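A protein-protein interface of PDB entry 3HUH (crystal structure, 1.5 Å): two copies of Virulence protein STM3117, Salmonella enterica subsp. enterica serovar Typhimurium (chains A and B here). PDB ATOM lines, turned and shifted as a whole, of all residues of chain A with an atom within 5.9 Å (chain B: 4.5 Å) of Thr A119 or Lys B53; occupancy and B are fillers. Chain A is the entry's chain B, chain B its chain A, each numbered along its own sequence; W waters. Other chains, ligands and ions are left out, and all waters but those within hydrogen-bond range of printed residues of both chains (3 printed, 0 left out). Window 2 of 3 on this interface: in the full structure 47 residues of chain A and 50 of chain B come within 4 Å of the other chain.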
ATOM      1  N   GLU A 117     -26.520  25.954 -31.062  1.00  0.00           N
ATOM      2  CA  GLU A 117     -27.083  24.764 -31.681  1.00  0.00           C
ATOM      3  C   GLU A 117     -26.744  23.543 -30.835  1.00  0.00           C
ATOM      4  O   GLU A 117     -25.614  23.381 -30.378  1.00  0.00           O
ATOM      5  CB  GLU A 117     -26.531  24.573 -33.095  1.00  0.00           C
ATOM      6  CG  GLU A 117     -26.719  25.766 -34.006  1.00  0.00           C
ATOM      7  CD  GLU A 117     -25.505  26.674 -34.025  1.00  0.00           C
ATOM      8  OE1 GLU A 117     -25.167  27.259 -32.973  1.00  0.00           O
ATOM      9  OE2 GLU A 117     -24.880  26.797 -35.102  1.00  0.00           O
ATOM     10  N   ARG A 118     -27.737  22.693 -30.625  1.00  0.00           N
ATOM     11  CA  ARG A 118     -27.562  21.486 -29.835  1.00  0.00           C
ATOM     12  C   ARG A 118     -28.399  20.389 -30.464  1.00  0.00           C
ATOM     13  O   ARG A 118     -29.179  20.637 -31.386  1.00  0.00           O
ATOM     14  CB  ARG A 118     -28.021  21.722 -28.389  1.00  0.00           C
ATOM     15  CG  ARG A 118     -27.089  22.603 -27.562  1.00  0.00           C
ATOM     16  CD  ARG A 118     -25.894  21.808 -27.048  1.00  0.00           C
ATOM     17  NE  ARG A 118     -24.937  22.633 -26.315  1.00  0.00           N
ATOM     18  CZ  ARG A 118     -24.038  23.427 -26.889  1.00  0.00           C
ATOM     19  NH1 ARG A 118     -23.967  23.506 -28.208  1.00  0.00           N
ATOM     20  NH2 ARG A 118     -23.206  24.143 -26.145  1.00  0.00           N
ATOM     21  N   THR A 119     -28.236  19.174 -29.964  1.00  0.00           N
ATOM     22  CA  THR A 119     -28.992  18.047 -30.479  1.00  0.00           C
ATOM     23  C   THR A 119     -30.229  17.792 -29.622  1.00  0.00           C
ATOM     24  O   THR A 119     -30.125  17.541 -28.421  1.00  0.00           O
ATOM     25  CB  THR A 119     -28.132  16.774 -30.497  1.00  0.00           C
ATOM     26  OG1 THR A 119     -27.680  16.491 -29.168  1.00  0.00           O
ATOM     27  CG2 THR A 119     -26.918  16.962 -31.405  1.00  0.00           C
ATOM     28  N   GLY A 120     -31.399  17.877 -30.241  1.00  0.00           N
ATOM     29  CA  GLY A 120     -32.629  17.625 -29.519  1.00  0.00           C
ATOM     30  C   GLY A 120     -32.946  16.150 -29.632  1.00  0.00           C
ATOM     31  O   GLY A 120     -32.229  15.411 -30.319  1.00  0.00           O
ATOM     32  N   ALA A 121     -34.013  15.720 -28.968  1.00  0.00           N
ATOM     33  CA  ALA A 121     -34.421  14.322 -28.993  1.00  0.00           C
ATOM     34  C   ALA A 121     -34.770  13.827 -30.397  1.00  0.00           C
ATOM     35  O   ALA A 121     -34.661  12.634 -30.682  1.00  0.00           O
ATOM     36  CB  ALA A 121     -35.610  14.122 -28.069  1.00  0.00           C
ATOM     37  N   GLY A 123     -33.967  15.981 -33.420  1.00  0.00           N
ATOM     38  CA  GLY A 123     -33.337  16.805 -34.433  1.00  0.00           C
ATOM     39  C   GLY A 123     -32.568  17.960 -33.826  1.00  0.00           C
ATOM     40  O   GLY A 123     -32.391  18.027 -32.608  1.00  0.00           O
ATOM     41  N   GLU A 124     -32.106  18.872 -34.673  1.00  0.00           N
ATOM     42  CA  GLU A 124     -31.353  20.018 -34.193  1.00  0.00           C
ATOM     43  C   GLU A 124     -32.268  21.046 -33.541  1.00  0.00           C
ATOM     44  O   GLU A 124     -33.400  21.263 -33.980  1.00  0.00           O
ATOM     45  CB  GLU A 124     -30.571  20.666 -35.343  1.00  0.00           C
ATOM     46  CG  GLU A 124     -29.823  21.936 -34.935  1.00  0.00           C
ATOM     47  CD  GLU A 124     -28.884  22.447 -36.016  1.00  0.00           C
ATOM     48  OE1 GLU A 124     -27.816  21.833 -36.218  1.00  0.00           O
ATOM     49  OE2 GLU A 124     -29.216  23.461 -36.666  1.00  0.00           O
ATOM     50  N   ILE A 125     -31.764  21.657 -32.477  1.00  0.00           N
ATOM     51  CA  ILE A 125     -32.495  22.677 -31.736  1.00  0.00           C
ATOM     52  C   ILE A 125     -31.536  23.826 -31.438  1.00  0.00           C
ATOM     53  O   ILE A 125     -30.323  23.668 -31.524  1.00  0.00           O
ATOM     54  CB  ILE A 125     -33.034  22.119 -30.374  1.00  0.00           C
ATOM     55  CG1 ILE A 125     -31.866  21.638 -29.503  1.00  0.00           C
ATOM     56  CG2 ILE A 125     -34.019  20.978 -30.615  1.00  0.00           C
ATOM     57  CD1 ILE A 125     -32.275  21.138 -28.107  1.00  0.00           C
ATOM     58  N   GLU A 139     -32.464  24.238 -19.870  1.00  0.00           N
ATOM     59  CA  GLU A 139     -32.207  24.458 -21.290  1.00  0.00           C
ATOM     60  C   GLU A 139     -33.547  24.708 -21.976  1.00  0.00           C
ATOM     61  O   GLU A 139     -34.420  23.840 -21.990  1.00  0.00           O
ATOM     62  CB  GLU A 139     -31.525  23.210 -21.879  1.00  0.00           C
ATOM     63  CG  GLU A 139     -31.184  23.267 -23.364  1.00  0.00           C
ATOM     64  CD  GLU A 139     -30.520  21.984 -23.861  1.00  0.00           C
ATOM     65  OE1 GLU A 139     -30.410  21.011 -23.078  1.00  0.00           O
ATOM     66  OE2 GLU A 139     -30.114  21.945 -25.040  1.00  0.00           O
ATOM     67  N   HIS B  26     -35.674  16.568 -23.222  1.00  0.00           N
ATOM     68  CA  HIS B  26     -34.711  15.627 -22.686  1.00  0.00           C
ATOM     69  C   HIS B  26     -34.209  16.118 -21.344  1.00  0.00           C
ATOM     70  O   HIS B  26     -34.576  17.202 -20.884  1.00  0.00           O
ATOM     71  CB  HIS B  26     -33.533  15.467 -23.663  1.00  0.00           C
ATOM     72  CG  HIS B  26     -32.808  16.745 -23.974  1.00  0.00           C
ATOM     73  ND1 HIS B  26     -31.840  17.280 -23.150  1.00  0.00           N
ATOM     74  CD2 HIS B  26     -32.894  17.578 -25.040  1.00  0.00           C
ATOM     75  CE1 HIS B  26     -31.357  18.383 -23.698  1.00  0.00           C
ATOM     76  NE2 HIS B  26     -31.981  18.586 -24.845  1.00  0.00           N
ATOM     77  N   PHE B  52     -24.211  10.324 -29.840  1.00  0.00           N
ATOM     78  CA  PHE B  52     -24.298  11.581 -30.567  1.00  0.00           C
ATOM     79  C   PHE B  52     -23.075  12.432 -30.240  1.00  0.00           C
ATOM     80  O   PHE B  52     -22.348  12.144 -29.288  1.00  0.00           O
ATOM     81  CB  PHE B  52     -25.594  12.323 -30.211  1.00  0.00           C
ATOM     82  CG  PHE B  52     -25.644  12.837 -28.800  1.00  0.00           C
ATOM     83  CD1 PHE B  52     -25.335  14.163 -28.524  1.00  0.00           C
ATOM     84  CD2 PHE B  52     -26.032  12.004 -27.750  1.00  0.00           C
ATOM     85  CE1 PHE B  52     -25.412  14.663 -27.229  1.00  0.00           C
ATOM     86  CE2 PHE B  52     -26.114  12.495 -26.444  1.00  0.00           C
ATOM     87  CZ  PHE B  52     -25.804  13.830 -26.185  1.00  0.00           C
ATOM     88  N   LYS B  53     -22.850  13.478 -31.028  1.00  0.00           N
ATOM     89  CA  LYS B  53     -21.694  14.339 -30.822  1.00  0.00           C
ATOM     90  C   LYS B  53     -20.424  13.495 -30.741  1.00  0.00           C
ATOM     91  O   LYS B  53     -19.558  13.731 -29.903  1.00  0.00           O
ATOM     92  CB  LYS B  53     -21.856  15.169 -29.547  1.00  0.00           C
ATOM     93  CG  LYS B  53     -22.260  16.617 -29.795  1.00  0.00           C
ATOM     94  CD  LYS B  53     -23.592  16.721 -30.521  1.00  0.00           C
ATOM     95  CE  LYS B  53     -23.954  18.173 -30.807  1.00  0.00           C
ATOM     96  NZ  LYS B  53     -23.037  18.812 -31.795  1.00  0.00           N
ATOM     97  N   GLN B  54     -20.348  12.495 -31.616  1.00  0.00           N
ATOM     98  CA  GLN B  54     -19.206  11.588 -31.723  1.00  0.00           C
ATOM     99  C   GLN B  54     -18.948  10.577 -30.607  1.00  0.00           C
ATOM    100  O   GLN B  54     -18.618   9.425 -30.886  1.00  0.00           O
ATOM    101  CB  GLN B  54     -17.913  12.386 -31.949  1.00  0.00           C
ATOM    102  CG  GLN B  54     -16.674  11.499 -32.045  1.00  0.00           C
ATOM    103  CD  GLN B  54     -15.375  12.285 -32.136  1.00  0.00           C
ATOM    104  OE1 GLN B  54     -15.029  13.055 -31.237  1.00  0.00           O
ATOM    105  NE2 GLN B  54     -14.645  12.087 -33.228  1.00  0.00           N
ATOM    106  N   ASN B  55     -19.090  10.988 -29.350  1.00  0.00           N
ATOM    107  CA  ASN B  55     -18.798  10.080 -28.245  1.00  0.00           C
ATOM    108  C   ASN B  55     -19.719  10.167 -27.026  1.00  0.00           C
ATOM    109  O   ASN B  55     -19.401   9.616 -25.974  1.00  0.00           O
ATOM    110  CB  ASN B  55     -17.360  10.312 -27.775  1.00  0.00           C
ATOM    111  CG  ASN B  55     -17.093  11.775 -27.466  1.00  0.00           C
ATOM    112  OD1 ASN B  55     -17.999  12.503 -27.061  1.00  0.00           O
ATOM    113  ND2 ASN B  55     -15.853  12.208 -27.649  1.00  0.00           N
ATOM    114  N   ARG B  56     -20.853  10.843 -27.157  1.00  0.00           N
ATOM    115  CA  ARG B  56     -21.770  10.972 -26.031  1.00  0.00           C
ATOM    116  C   ARG B  56     -22.901   9.963 -26.131  1.00  0.00           C
ATOM    117  O   ARG B  56     -23.317   9.599 -27.232  1.00  0.00           O
ATOM    118  CB  ARG B  56     -22.333  12.388 -25.983  1.00  0.00           C
ATOM    119  CG  ARG B  56     -21.249  13.456 -26.009  1.00  0.00           C
ATOM    120  CD  ARG B  56     -21.798  14.770 -25.555  1.00  0.00           C
ATOM    121  NE  ARG B  56     -20.811  15.837 -25.668  1.00  0.00           N
ATOM    122  CZ  ARG B  56     -21.017  17.071 -25.231  1.00  0.00           C
ATOM    123  NH1 ARG B  56     -22.171  17.375 -24.648  1.00  0.00           N
ATOM    124  NH2 ARG B  56     -20.084  18.005 -25.397  1.00  0.00           N
ATOM    125  N   LYS B  65     -35.590  11.923 -25.009  1.00  0.00           N
ATOM    126  CA  LYS B  65     -34.369  11.185 -24.729  1.00  0.00           C
ATOM    127  C   LYS B  65     -33.746  11.590 -23.405  1.00  0.00           C
ATOM    128  O   LYS B  65     -34.066  12.640 -22.848  1.00  0.00           O
ATOM    129  CB  LYS B  65     -33.339  11.351 -25.858  1.00  0.00           C
ATOM    130  CG  LYS B  65     -32.680  12.726 -25.971  1.00  0.00           C
ATOM    131  CD  LYS B  65     -31.466  12.645 -26.904  1.00  0.00           C
ATOM    132  CE  LYS B  65     -30.837  14.012 -27.142  1.00  0.00           C
ATOM    133  NZ  LYS B  65     -29.400  13.859 -27.530  1.00  0.00           N
HETATM  134  O   HOH W   1     -30.359  19.125 -20.716  1.00  0.00           O
HETATM  135  O   HOH W   2     -28.338  16.295 -26.703  1.00  0.00           O
HETATM  136  O   HOH W   3     -28.723  19.527 -25.355  1.00  0.00           O
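Printed residues of chain A that touch a printed residue of chain B: Thr A119, Gly A120, Ala A121 and Glu A139. Hydrophobic or aromatic side chains of chain A that line the printed part of chain B: Ala A121. Of the 7 printed residues of chain B, 4 touch a printed residue of chain A. Among the printed residues, 6 pairs touch across the chains.
A ring nitrogen (NE2) of His B26 lies close to the side-chain carboxylate (OE1) of Glu A139 (3.4 Å).
No position is printed for both chains. Of the 6 pairs that touch across the chains among the printed residues, none has its exchanged pair printed and touching as well.
OD1 of Asn B55 lies close to O of Lys B53, at 3.5 Å.
Thr A119 touches Phe B52. CE of Lys B53 touches CG2 of Thr A119, at 3.3 Å. NZ of Lys B65 touches OG1 of Thr A119, at 3.5 Å. CE of Lys B65 touches O of Gly A120 (3.7 Å). Ala A121 touches Lys B65.
Of chain B, only Phe B52 (3.4 Å), Lys B53 (3.3 Å) and Lys B65 (3.5 Å) come within 4 Å of Thr A119. Lys B53 touches one residue of chain A. Printed residues of chain A within 4 Å of His B26: Glu A139. Of the printed residues of chain B, Ala A121 touches Lys B65. Of the printed residues of chain A, Phe B52 touches Thr A119 (3.4 Å). Of the printed residues of chain A, Lys B65 touches Thr A119, Gly A120 and Ala A121. The nearest residue of chain B that does not touch Thr A119 is His B26 (4.2 Å). The nearest printed residue of chain B that does not touch Ala A121 is His B26 (4.5 Å).
Water W2 bridges OG1 of Thr A119 and NZ of Lys B65. Water W3 bridges OE2 of Glu A139 and NE2 of His B26. Water W1 bridges OE1 of Glu A139 (3.0 Å) and ND1 of His B26 (3.4 Å).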
